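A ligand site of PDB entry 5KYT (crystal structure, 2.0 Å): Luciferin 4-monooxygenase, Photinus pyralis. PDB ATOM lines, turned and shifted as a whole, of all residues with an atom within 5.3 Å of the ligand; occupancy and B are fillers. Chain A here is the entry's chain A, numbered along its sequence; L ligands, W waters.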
ATOM      1  N   SER A 199      31.122 -24.375  30.687  1.00  0.00           N
ATOM      2  CA  SER A 199      31.663 -24.547  29.348  1.00  0.00           C
ATOM      3  C   SER A 199      32.898 -25.448  29.362  1.00  0.00           C
ATOM      4  O   SER A 199      32.965 -26.448  28.644  1.00  0.00           O
ATOM      5  CB  SER A 199      32.006 -23.184  28.752  1.00  0.00           C
ATOM      6  OG  SER A 199      32.713 -23.334  27.528  1.00  0.00           O
ATOM      7  N   ARG A 218      16.041 -14.848  39.207  1.00  0.00           N
ATOM      8  CA  ARG A 218      15.672 -14.987  37.786  1.00  0.00           C
ATOM      9  C   ARG A 218      14.177 -14.723  37.569  1.00  0.00           C
ATOM     10  O   ARG A 218      13.785 -14.109  36.576  1.00  0.00           O
ATOM     11  CB  ARG A 218      16.027 -16.391  37.260  1.00  0.00           C
ATOM     12  CG  ARG A 218      15.430 -16.711  35.892  1.00  0.00           C
ATOM     13  CD  ARG A 218      15.953 -15.797  34.793  1.00  0.00           C
ATOM     14  NE  ARG A 218      15.211 -15.944  33.541  1.00  0.00           N
ATOM     15  CZ  ARG A 218      15.208 -15.030  32.560  1.00  0.00           C
ATOM     16  NH1 ARG A 218      15.899 -13.900  32.674  1.00  0.00           N
ATOM     17  NH2 ARG A 218      14.509 -15.246  31.449  1.00  0.00           N
ATOM     18  N   HIS A 245      20.982 -26.541  29.395  1.00  0.00           N
ATOM     19  CA  HIS A 245      21.926 -25.420  29.457  1.00  0.00           C
ATOM     20  C   HIS A 245      21.270 -24.262  30.199  1.00  0.00           C
ATOM     21  O   HIS A 245      20.043 -24.140  30.180  1.00  0.00           O
ATOM     22  CB  HIS A 245      22.314 -25.013  28.029  1.00  0.00           C
ATOM     23  CG  HIS A 245      23.371 -23.953  27.931  1.00  0.00           C
ATOM     24  ND1 HIS A 245      23.062 -22.609  27.851  1.00  0.00           N
ATOM     25  CD2 HIS A 245      24.720 -24.044  27.834  1.00  0.00           C
ATOM     26  CE1 HIS A 245      24.186 -21.917  27.729  1.00  0.00           C
ATOM     27  NE2 HIS A 245      25.194 -22.764  27.724  1.00  0.00           N
ATOM     28  N   GLY A 246      22.076 -23.412  30.833  1.00  0.00           N
ATOM     29  CA  GLY A 246      21.565 -22.254  31.549  1.00  0.00           C
ATOM     30  C   GLY A 246      20.602 -21.369  30.759  1.00  0.00           C
ATOM     31  O   GLY A 246      19.594 -20.920  31.295  1.00  0.00           O
ATOM     32  N   PHE A 247      20.914 -21.134  29.492  1.00  0.00           N
ATOM     33  CA  PHE A 247      20.055 -20.351  28.600  1.00  0.00           C
ATOM     34  C   PHE A 247      18.635 -20.938  28.535  1.00  0.00           C
ATOM     35  O   PHE A 247      17.645 -20.212  28.708  1.00  0.00           O
ATOM     36  CB  PHE A 247      20.696 -20.266  27.214  1.00  0.00           C
ATOM     37  CG  PHE A 247      20.013 -19.302  26.259  1.00  0.00           C
ATOM     38  CD1 PHE A 247      19.039 -18.424  26.688  1.00  0.00           C
ATOM     39  CD2 PHE A 247      20.360 -19.316  24.911  1.00  0.00           C
ATOM     40  CE1 PHE A 247      18.414 -17.554  25.780  1.00  0.00           C
ATOM     41  CE2 PHE A 247      19.752 -18.449  24.003  1.00  0.00           C
ATOM     42  CZ  PHE A 247      18.778 -17.571  24.432  1.00  0.00           C
ATOM     43  N   THR A 251      15.338 -19.610  31.104  1.00  0.00           N
ATOM     44  CA  THR A 251      14.274 -18.952  30.345  1.00  0.00           C
ATOM     45  C   THR A 251      12.996 -19.749  30.500  1.00  0.00           C
ATOM     46  O   THR A 251      11.933 -19.183  30.751  1.00  0.00           O
ATOM     47  CB  THR A 251      14.588 -18.792  28.850  1.00  0.00           C
ATOM     48  OG1 THR A 251      14.968 -20.057  28.288  1.00  0.00           O
ATOM     49  CG2 THR A 251      15.709 -17.737  28.638  1.00  0.00           C
ATOM     50  N   LEU A 286      12.762 -17.565  20.813  1.00  0.00           N
ATOM     51  CA  LEU A 286      14.026 -17.603  21.512  1.00  0.00           C
ATOM     52  C   LEU A 286      15.021 -18.425  20.710  1.00  0.00           C
ATOM     53  O   LEU A 286      14.886 -19.636  20.613  1.00  0.00           O
ATOM     54  CB  LEU A 286      13.838 -18.189  22.920  1.00  0.00           C
ATOM     55  CG  LEU A 286      15.028 -18.041  23.849  1.00  0.00           C
ATOM     56  CD1 LEU A 286      15.179 -16.564  24.226  1.00  0.00           C
ATOM     57  CD2 LEU A 286      14.877 -18.922  25.086  1.00  0.00           C
ATOM     58  N   ALA A 313      14.487 -13.143  20.323  1.00  0.00           N
ATOM     59  CA  ALA A 313      15.540 -12.945  21.316  1.00  0.00           C
ATOM     60  C   ALA A 313      16.690 -13.917  21.069  1.00  0.00           C
ATOM     61  O   ALA A 313      16.459 -15.102  20.836  1.00  0.00           O
ATOM     62  CB  ALA A 313      14.991 -13.129  22.724  1.00  0.00           C
ATOM     63  N   SER A 314      17.911 -13.408  21.123  1.00  0.00           N
ATOM     64  CA  SER A 314      19.096 -14.248  20.967  1.00  0.00           C
ATOM     65  C   SER A 314      19.969 -14.206  22.231  1.00  0.00           C
ATOM     66  O   SER A 314      19.920 -13.250  22.989  1.00  0.00           O
ATOM     67  CB  SER A 314      19.909 -13.792  19.745  1.00  0.00           C
ATOM     68  OG  SER A 314      21.011 -14.650  19.503  1.00  0.00           O
ATOM     69  N   GLY A 315      20.759 -15.254  22.429  1.00  0.00           N
ATOM     70  CA  GLY A 315      21.716 -15.262  23.514  1.00  0.00           C
ATOM     71  C   GLY A 315      22.750 -16.373  23.363  1.00  0.00           C
ATOM     72  O   GLY A 315      22.680 -17.164  22.417  1.00  0.00           O
ATOM     73  N   GLY A 316      23.700 -16.425  24.293  1.00  0.00           N
ATOM     74  CA  GLY A 316      24.595 -17.569  24.402  1.00  0.00           C
ATOM     75  C   GLY A 316      25.809 -17.538  23.493  1.00  0.00           C
ATOM     76  O   GLY A 316      26.736 -18.314  23.654  1.00  0.00           O
ATOM     77  N   ALA A 317      25.813 -16.625  22.528  1.00  0.00           N
ATOM     78  CA  ALA A 317      26.950 -16.484  21.605  1.00  0.00           C
ATOM     79  C   ALA A 317      26.852 -15.151  20.911  1.00  0.00           C
ATOM     80  O   ALA A 317      25.794 -14.524  20.945  1.00  0.00           O
ATOM     81  CB  ALA A 317      26.982 -17.626  20.572  1.00  0.00           C
ATOM     82  N   PRO A 318      27.938 -14.712  20.257  1.00  0.00           N
ATOM     83  CA  PRO A 318      27.924 -13.435  19.527  1.00  0.00           C
ATOM     84  C   PRO A 318      26.922 -13.435  18.379  1.00  0.00           C
ATOM     85  O   PRO A 318      26.774 -14.439  17.691  1.00  0.00           O
ATOM     86  CB  PRO A 318      29.361 -13.310  18.987  1.00  0.00           C
ATOM     87  CG  PRO A 318      30.181 -14.224  19.820  1.00  0.00           C
ATOM     88  CD  PRO A 318      29.258 -15.348  20.236  1.00  0.00           C
ATOM     89  N   LEU A 319      26.242 -12.310  18.170  1.00  0.00           N
ATOM     90  CA  LEU A 319      25.436 -12.111  16.971  1.00  0.00           C
ATOM     91  C   LEU A 319      25.985 -10.895  16.236  1.00  0.00           C
ATOM     92  O   LEU A 319      26.028  -9.813  16.801  1.00  0.00           O
ATOM     93  CB  LEU A 319      23.968 -11.913  17.325  1.00  0.00           C
ATOM     94  CG  LEU A 319      22.999 -11.561  16.173  1.00  0.00           C
ATOM     95  CD1 LEU A 319      22.809 -12.735  15.227  1.00  0.00           C
ATOM     96  CD2 LEU A 319      21.657 -11.121  16.724  1.00  0.00           C
ATOM     97  N   GLN A 338      18.651  -9.086  22.898  1.00  0.00           N
ATOM     98  CA  GLN A 338      19.837  -9.846  23.305  1.00  0.00           C
ATOM     99  C   GLN A 338      19.802 -10.125  24.776  1.00  0.00           C
ATOM    100  O   GLN A 338      19.256  -9.340  25.558  1.00  0.00           O
ATOM    101  CB  GLN A 338      21.148  -9.098  23.010  1.00  0.00           C
ATOM    102  CG  GLN A 338      21.530  -8.926  21.557  1.00  0.00           C
ATOM    103  CD  GLN A 338      22.202 -10.141  20.961  1.00  0.00           C
ATOM    104  OE1 GLN A 338      23.008 -10.820  21.617  1.00  0.00           O
ATOM    105  NE2 GLN A 338      21.870 -10.434  19.700  1.00  0.00           N
ATOM    106  N   GLY A 339      20.435 -11.226  25.166  1.00  0.00           N
ATOM    107  CA  GLY A 339      20.797 -11.443  26.550  1.00  0.00           C
ATOM    108  C   GLY A 339      22.173 -12.072  26.599  1.00  0.00           C
ATOM    109  O   GLY A 339      22.492 -12.917  25.775  1.00  0.00           O
ATOM    110  N   TYR A 340      22.981 -11.624  27.552  1.00  0.00           N
ATOM    111  CA  TYR A 340      24.307 -12.171  27.775  1.00  0.00           C
ATOM    112  C   TYR A 340      24.379 -12.703  29.198  1.00  0.00           C
ATOM    113  O   TYR A 340      23.963 -12.041  30.159  1.00  0.00           O
ATOM    114  CB  TYR A 340      25.385 -11.111  27.524  1.00  0.00           C
ATOM    115  CG  TYR A 340      26.733 -11.397  28.185  1.00  0.00           C
ATOM    116  CD1 TYR A 340      26.958 -11.065  29.529  1.00  0.00           C
ATOM    117  CD2 TYR A 340      27.780 -11.975  27.473  1.00  0.00           C
ATOM    118  CE1 TYR A 340      28.169 -11.311  30.134  1.00  0.00           C
ATOM    119  CE2 TYR A 340      29.018 -12.239  28.086  1.00  0.00           C
ATOM    120  CZ  TYR A 340      29.195 -11.901  29.399  1.00  0.00           C
ATOM    121  OH  TYR A 340      30.407 -12.140  29.992  1.00  0.00           O
ATOM    122  N   GLY A 341      24.883 -13.925  29.330  1.00  0.00           N
ATOM    123  CA  GLY A 341      25.113 -14.503  30.645  1.00  0.00           C
ATOM    124  C   GLY A 341      26.112 -15.642  30.581  1.00  0.00           C
ATOM    125  O   GLY A 341      26.598 -15.987  29.500  1.00  0.00           O
ATOM    126  N   LEU A 342      26.452 -16.217  31.740  1.00  0.00           N
ATOM    127  CA  LEU A 342      27.263 -17.435  31.804  1.00  0.00           C
ATOM    128  C   LEU A 342      26.561 -18.434  32.703  1.00  0.00           C
ATOM    129  O   LEU A 342      25.733 -18.071  33.530  1.00  0.00           O
ATOM    130  CB  LEU A 342      28.677 -17.161  32.351  1.00  0.00           C
ATOM    131  CG  LEU A 342      29.623 -16.188  31.633  1.00  0.00           C
ATOM    132  CD1 LEU A 342      29.246 -14.742  31.915  1.00  0.00           C
ATOM    133  CD2 LEU A 342      31.054 -16.440  32.081  1.00  0.00           C
ATOM    134  N   THR A 343      26.905 -19.708  32.548  1.00  0.00           N
ATOM    135  CA  THR A 343      26.319 -20.731  33.405  1.00  0.00           C
ATOM    136  C   THR A 343      26.496 -20.327  34.877  1.00  0.00           C
ATOM    137  O   THR A 343      25.566 -20.457  35.692  1.00  0.00           O
ATOM    138  CB  THR A 343      26.954 -22.107  33.147  1.00  0.00           C
ATOM    139  OG1 THR A 343      26.773 -22.446  31.761  1.00  0.00           O
ATOM    140  CG2 THR A 343      26.295 -23.162  34.033  1.00  0.00           C
ATOM    141  N   GLU A 344      27.654 -19.762  35.171  1.00  0.00           N
ATOM    142  CA  GLU A 344      28.020 -19.344  36.511  1.00  0.00           C
ATOM    143  C   GLU A 344      27.285 -18.086  36.991  1.00  0.00           C
ATOM    144  O   GLU A 344      27.394 -17.727  38.152  1.00  0.00           O
ATOM    145  CB  GLU A 344      29.545 -19.122  36.588  1.00  0.00           C
ATOM    146  CG  GLU A 344      30.391 -20.399  36.442  1.00  0.00           C
ATOM    147  CD  GLU A 344      30.805 -20.696  35.012  1.00  0.00           C
ATOM    148  OE1 GLU A 344      30.083 -20.240  34.089  1.00  0.00           O
ATOM    149  OE2 GLU A 344      31.837 -21.364  34.800  1.00  0.00           O
ATOM    150  N   THR A 346      23.979 -17.977  36.498  1.00  0.00           N
ATOM    151  CA  THR A 346      22.624 -18.516  36.421  1.00  0.00           C
ATOM    152  C   THR A 346      21.921 -18.213  35.097  1.00  0.00           C
ATOM    153  O   THR A 346      21.567 -19.131  34.353  1.00  0.00           O
ATOM    154  CB  THR A 346      21.709 -18.008  37.569  1.00  0.00           C
ATOM    155  OG1 THR A 346      22.268 -18.362  38.843  1.00  0.00           O
ATOM    156  CG2 THR A 346      20.307 -18.649  37.450  1.00  0.00           C
ATOM    157  N   SER A 347      21.677 -16.924  34.827  1.00  0.00           N
ATOM    158  CA  SER A 347      20.943 -16.514  33.626  1.00  0.00           C
ATOM    159  C   SER A 347      21.598 -15.253  33.050  1.00  0.00           C
ATOM    160  O   SER A 347      22.731 -14.927  33.412  1.00  0.00           O
ATOM    161  CB  SER A 347      19.444 -16.276  33.945  1.00  0.00           C
ATOM    162  OG  SER A 347      18.669 -16.103  32.757  1.00  0.00           O
ATOM    163  N   ALA A 348      20.920 -14.547  32.138  1.00  0.00           N
ATOM    164  CA  ALA A 348      21.491 -13.339  31.537  1.00  0.00           C
ATOM    165  C   ALA A 348      21.583 -12.221  32.569  1.00  0.00           C
ATOM    166  O   ALA A 348      20.628 -11.992  33.318  1.00  0.00           O
ATOM    167  CB  ALA A 348      20.643 -12.876  30.354  1.00  0.00           C
ATOM    168  N   ILE A 351      20.907  -7.574  29.603  1.00  0.00           N
ATOM    169  CA  ILE A 351      19.742  -7.782  28.755  1.00  0.00           C
ATOM    170  C   ILE A 351      19.346  -6.455  28.086  1.00  0.00           C
ATOM    171  O   ILE A 351      19.401  -5.389  28.708  1.00  0.00           O
ATOM    172  CB  ILE A 351      18.552  -8.332  29.570  1.00  0.00           C
ATOM    173  CG1 ILE A 351      18.885  -9.707  30.168  1.00  0.00           C
ATOM    174  CG2 ILE A 351      17.293  -8.369  28.691  1.00  0.00           C
ATOM    175  CD1 ILE A 351      17.875 -10.209  31.186  1.00  0.00           C
ATOM    176  N   VAL A 362      24.726  -6.014  23.699  1.00  0.00           N
ATOM    177  CA  VAL A 362      24.043  -7.156  24.317  1.00  0.00           C
ATOM    178  C   VAL A 362      23.064  -6.660  25.390  1.00  0.00           C
ATOM    179  O   VAL A 362      22.338  -7.453  25.990  1.00  0.00           O
ATOM    180  CB  VAL A 362      25.035  -8.184  24.939  1.00  0.00           C
ATOM    181  CG1 VAL A 362      25.796  -8.919  23.837  1.00  0.00           C
ATOM    182  CG2 VAL A 362      25.990  -7.507  25.936  1.00  0.00           C
ATOM    183  N   SER A 420      34.598 -12.890  33.912  1.00  0.00           N
ATOM    184  CA  SER A 420      33.945 -13.640  32.853  1.00  0.00           C
ATOM    185  C   SER A 420      34.865 -14.269  31.816  1.00  0.00           C
ATOM    186  O   SER A 420      34.475 -15.209  31.123  1.00  0.00           O
ATOM    187  CB  SER A 420      32.978 -12.725  32.104  1.00  0.00           C
ATOM    188  OG  SER A 420      33.713 -11.779  31.339  1.00  0.00           O
ATOM    189  N   ASP A 422      35.559 -12.624  29.236  1.00  0.00           N
ATOM    190  CA  ASP A 422      35.149 -11.911  28.030  1.00  0.00           C
ATOM    191  C   ASP A 422      35.723 -10.502  28.004  1.00  0.00           C
ATOM    192  O   ASP A 422      35.755  -9.826  29.022  1.00  0.00           O
ATOM    193  CB  ASP A 422      33.618 -11.811  27.939  1.00  0.00           C
ATOM    194  CG  ASP A 422      32.956 -13.161  27.736  1.00  0.00           C
ATOM    195  OD1 ASP A 422      33.421 -13.914  26.864  1.00  0.00           O
ATOM    196  OD2 ASP A 422      31.990 -13.467  28.453  1.00  0.00           O
ATOM    197  N   ILE A 434      30.082  -6.888  23.698  1.00  0.00           N
ATOM    198  CA  ILE A 434      31.032  -7.988  23.874  1.00  0.00           C
ATOM    199  C   ILE A 434      31.933  -8.053  22.656  1.00  0.00           C
ATOM    200  O   ILE A 434      31.458  -8.166  21.522  1.00  0.00           O
ATOM    201  CB  ILE A 434      30.321  -9.354  24.057  1.00  0.00           C
ATOM    202  CG1 ILE A 434      29.247  -9.267  25.126  1.00  0.00           C
ATOM    203  CG2 ILE A 434      31.342 -10.455  24.397  1.00  0.00           C
ATOM    204  CD1 ILE A 434      29.800  -9.111  26.555  1.00  0.00           C
ATOM    205  N   ARG A 437      35.660 -13.578  23.539  1.00  0.00           N
ATOM    206  CA  ARG A 437      36.377 -14.201  24.644  1.00  0.00           C
ATOM    207  C   ARG A 437      37.831 -13.772  24.534  1.00  0.00           C
ATOM    208  O   ARG A 437      38.408 -13.694  23.465  1.00  0.00           O
ATOM    209  CB  ARG A 437      36.216 -15.729  24.612  1.00  0.00           C
ATOM    210  CG  ARG A 437      34.825 -16.184  25.051  1.00  0.00           C
ATOM    211  CD  ARG A 437      34.568 -17.652  24.749  1.00  0.00           C
ATOM    212  NE  ARG A 437      34.388 -17.891  23.329  1.00  0.00           N
ATOM    213  CZ  ARG A 437      34.173 -19.083  22.785  1.00  0.00           C
ATOM    214  NH1 ARG A 437      34.096 -20.160  23.567  1.00  0.00           N
ATOM    215  NH2 ARG A 437      34.021 -19.210  21.477  1.00  0.00           N
ATOM    216  N   THR A 527      25.069 -23.827  21.633  1.00  0.00           N
ATOM    217  CA  THR A 527      24.516 -22.481  21.707  1.00  0.00           C
ATOM    218  C   THR A 527      25.103 -21.576  20.614  1.00  0.00           C
ATOM    219  O   THR A 527      24.654 -20.434  20.408  1.00  0.00           O
ATOM    220  CB  THR A 527      24.723 -21.853  23.127  1.00  0.00           C
ATOM    221  OG1 THR A 527      26.085 -22.009  23.545  1.00  0.00           O
ATOM    222  CG2 THR A 527      23.807 -22.554  24.143  1.00  0.00           C
ATOM    223  N   LYS A 529      28.656 -21.008  20.085  1.00  0.00           N
ATOM    224  CA  LYS A 529      30.032 -20.576  20.329  1.00  0.00           C
ATOM    225  C   LYS A 529      31.007 -21.396  19.455  1.00  0.00           C
ATOM    226  O   LYS A 529      30.924 -22.622  19.392  1.00  0.00           O
ATOM    227  CB  LYS A 529      30.388 -20.705  21.819  1.00  0.00           C
ATOM    228  CG  LYS A 529      29.611 -19.748  22.744  1.00  0.00           C
ATOM    229  CD  LYS A 529      29.988 -19.894  24.224  1.00  0.00           C
ATOM    230  CE  LYS A 529      28.929 -20.664  25.027  1.00  0.00           C
ATOM    231  NZ  LYS A 529      27.575 -19.985  25.176  1.00  0.00           N
HETATM  232  O1  LIG L   1      25.910 -18.929  27.371  1.00  0.00           O
HETATM  233  C1  LIG L   1      25.688 -19.079  28.543  1.00  0.00           C
HETATM  234  C2  LIG L   1      24.442 -18.588  29.126  1.00  0.00           C
HETATM  235  N1  LIG L   1      23.617 -17.799  28.457  1.00  0.00           N
HETATM  236  C3  LIG L   1      24.125 -18.986  30.407  1.00  0.00           C
HETATM  237  S1  LIG L   1      22.598 -18.209  30.685  1.00  0.00           S
HETATM  238  C4  LIG L   1      22.526 -17.466  29.096  1.00  0.00           C
HETATM  239  C5  LIG L   1      21.462 -16.624  28.650  1.00  0.00           C
HETATM  240  S2  LIG L   1      21.483 -15.672  27.157  1.00  0.00           S
HETATM  241  C6  LIG L   1      19.884 -14.991  27.436  1.00  0.00           C
HETATM  242  C7  LIG L   1      19.126 -14.127  26.706  1.00  0.00           C
HETATM  243  C8  LIG L   1      17.825 -13.917  27.107  1.00  0.00           C
HETATM  244  O2  LIG L   1      17.003 -13.217  26.283  1.00  0.00           O
HETATM  245  C9  LIG L   1      19.445 -15.558  28.658  1.00  0.00           C
HETATM  246  N2  LIG L   1      20.320 -16.384  29.243  1.00  0.00           N
HETATM  247  C10 LIG L   1      18.170 -15.194  29.130  1.00  0.00           C
HETATM  248  C11 LIG L   1      17.372 -14.425  28.337  1.00  0.00           C
HETATM  249  N3  LIG L   1      26.525 -19.717  29.369  1.00  0.00           N
HETATM  250  S3  LIG L   1      27.947 -20.339  28.865  1.00  0.00           S
HETATM  251  O3  LIG L   1      27.618 -21.532  28.130  1.00  0.00           O
HETATM  252  O4  LIG L   1      28.734 -20.300  30.026  1.00  0.00           O
HETATM  253  O5  LIG L   1      28.620 -19.460  27.817  1.00  0.00           O
HETATM  254  C12 LIG L   1      29.138 -18.304  28.449  1.00  0.00           C
HETATM  255  C13 LIG L   1      29.812 -17.447  27.357  1.00  0.00           C
HETATM  256  C14 LIG L   1      30.091 -15.981  27.756  1.00  0.00           C
HETATM  257  O6  LIG L   1      31.309 -15.897  28.497  1.00  0.00           O
HETATM  258  C15 LIG L   1      30.223 -15.300  26.375  1.00  0.00           C
HETATM  259  O7  LIG L   1      31.532 -15.535  25.840  1.00  0.00           O
HETATM  260  C16 LIG L   1      29.206 -16.080  25.504  1.00  0.00           C
HETATM  261  O8  LIG L   1      28.924 -17.307  26.219  1.00  0.00           O
HETATM  262  N4  LIG L   1      27.952 -15.342  25.342  1.00  0.00           N
HETATM  263  C17 LIG L   1      27.741 -14.296  24.476  1.00  0.00           C
HETATM  264  N5  LIG L   1      28.498 -13.641  23.589  1.00  0.00           N
HETATM  265  C18 LIG L   1      27.995 -12.642  22.888  1.00  0.00           C
HETATM  266  N6  LIG L   1      26.738 -12.243  22.998  1.00  0.00           N
HETATM  267  C19 LIG L   1      26.386 -13.903  24.644  1.00  0.00           C
HETATM  268  C20 LIG L   1      25.902 -12.829  23.863  1.00  0.00           C
HETATM  269  N7  LIG L   1      24.588 -12.386  23.980  1.00  0.00           N
HETATM  270  N8  LIG L   1      25.872 -14.713  25.606  1.00  0.00           N
HETATM  271  C21 LIG L   1      26.777 -15.553  26.022  1.00  0.00           C
HETATM  272  O   HOH W   1      25.931 -10.430  20.779  1.00  0.00           O
HETATM  273  O   HOH W   2      14.467 -12.763  27.121  1.00  0.00           O
HETATM  274  O   HOH W   3      31.386 -14.169  23.137  1.00  0.00           O
HETATM  275  O   HOH W   4      18.707 -18.237  31.025  1.00  0.00           O
HETATM  276  O   HOH W   5      30.505 -21.706  31.553  1.00  0.00           O
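The side-chain carboxylate (OD2) of Asp 422 sits at hydrogen-bond distance from an oxygen (O6) of the ligand (2.5 Å).
An oxygen (O3) of the ligand lies within hydrogen-bond range of a ring nitrogen (NE2) of His 245, 2.7 Å away.
N7 of the ligand lies within hydrogen-bond range of O of Gly 339 (2.8 Å).
The side-chain amino group of Lys 529 sits at hydrogen-bond distance from an oxygen (O5) of the ligand, at 2.9 Å.
A nitrogen (N8) of the ligand lies within hydrogen-bond range of the backbone NH (N) of Gly 316 (3.1 Å).
N of Thr 343 is in hydrogen-bond range of O4 of the ligand (3.2 Å).
An oxygen (O4) of the ligand lies within hydrogen-bond range of the side-chain hydroxyl (OG1) of Thr 343 (3.4 Å).
N7 of the ligand lies within hydrogen-bond range of OE1 of Gln 338.
The backbone NH of Phe 247 sits close to a sulfur (S1) of the ligand, 3.6 Å away.
N of Ala 348 is in hydrogen-bond range of N2 of the ligand.
The side-chain carboxylate of Asp 422 lies within hydrogen-bond range of the side-chain hydroxyl of Tyr 340, at 2.6 Å.
N of Asp 422 lies within hydrogen-bond range of OG of Ser 420, at 2.9 Å.
ND1 of His 245 is in hydrogen-bond range of N of Phe 247 (3.1 Å).
The backbone NH (N) of Gly 339 lies within hydrogen-bond range of the backbone carbonyl oxygen (O) of Ser 314, 3.0 Å away.
The side-chain amino group (NZ) of Lys 529 is in hydrogen-bond range of the backbone carbonyl oxygen (O) of Gly 316 (2.4 Å).
The side-chain amino group of Lys 529 is in hydrogen-bond range of the side-chain hydroxyl of Thr 527, at 3.0 Å.
O of Phe 247 sits at hydrogen-bond distance from OG1 of Thr 251, 2.7 Å away.
O of Ala 317 lies close to N6 of the ligand (3.2 Å).
Gly 246 touches the ligand (C to S1, 3.7 Å).
Thr 251 touches the ligand.
O of Ser 314 touches C7 of the ligand, at 3.9 Å.
Gly 315 touches the ligand (CA to S2, 3.7 Å).
Pro 318 touches the ligand (N to C18, 3.3 Å).
Tyr 340 touches the ligand.
Gly 341 touches the ligand (O to C1, 3.4 Å).
Leu 342 touches the ligand (C to C3, 3.4 Å).
O of Thr 346 touches S1 of the ligand, at 3.9 Å.
Ser 347 touches the ligand (OG to C10, 3.8 Å).
Val 362 touches the ligand.
Arg 437 touches the ligand (CG to O7, 3.4 Å).
Hydrophobic or aromatic side chains within 4 Å of the ligand: His 245, Phe 247, Pro 318, Tyr 340, Leu 342, Ala 348 and Val 362.
22 residues have an atom within 4 Å of the ligand: His 245, Gly 246, Phe 247, Thr 251, Ser 314, Gly 315, Gly 316, Ala 317, Pro 318, Gln 338, Gly 339, Tyr 340, Gly 341, Leu 342, Thr 343, Thr 346, Ser 347, Ala 348, Val 362, Asp 422, Arg 437 and Lys 529.
Water W5 lies within hydrogen-bond range of an oxygen (O4) of the ligand (2.7 Å), the backbone NH of Ser 199 (2.9 Å) and the side-chain carboxylate of Glu 344 (3.0 Å).
Water W1 lies within hydrogen-bond range of N6 of the ligand (3.0 Å), OE1 of Gln 338 (3.1 Å) and N of Leu 319 (3.2 Å).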
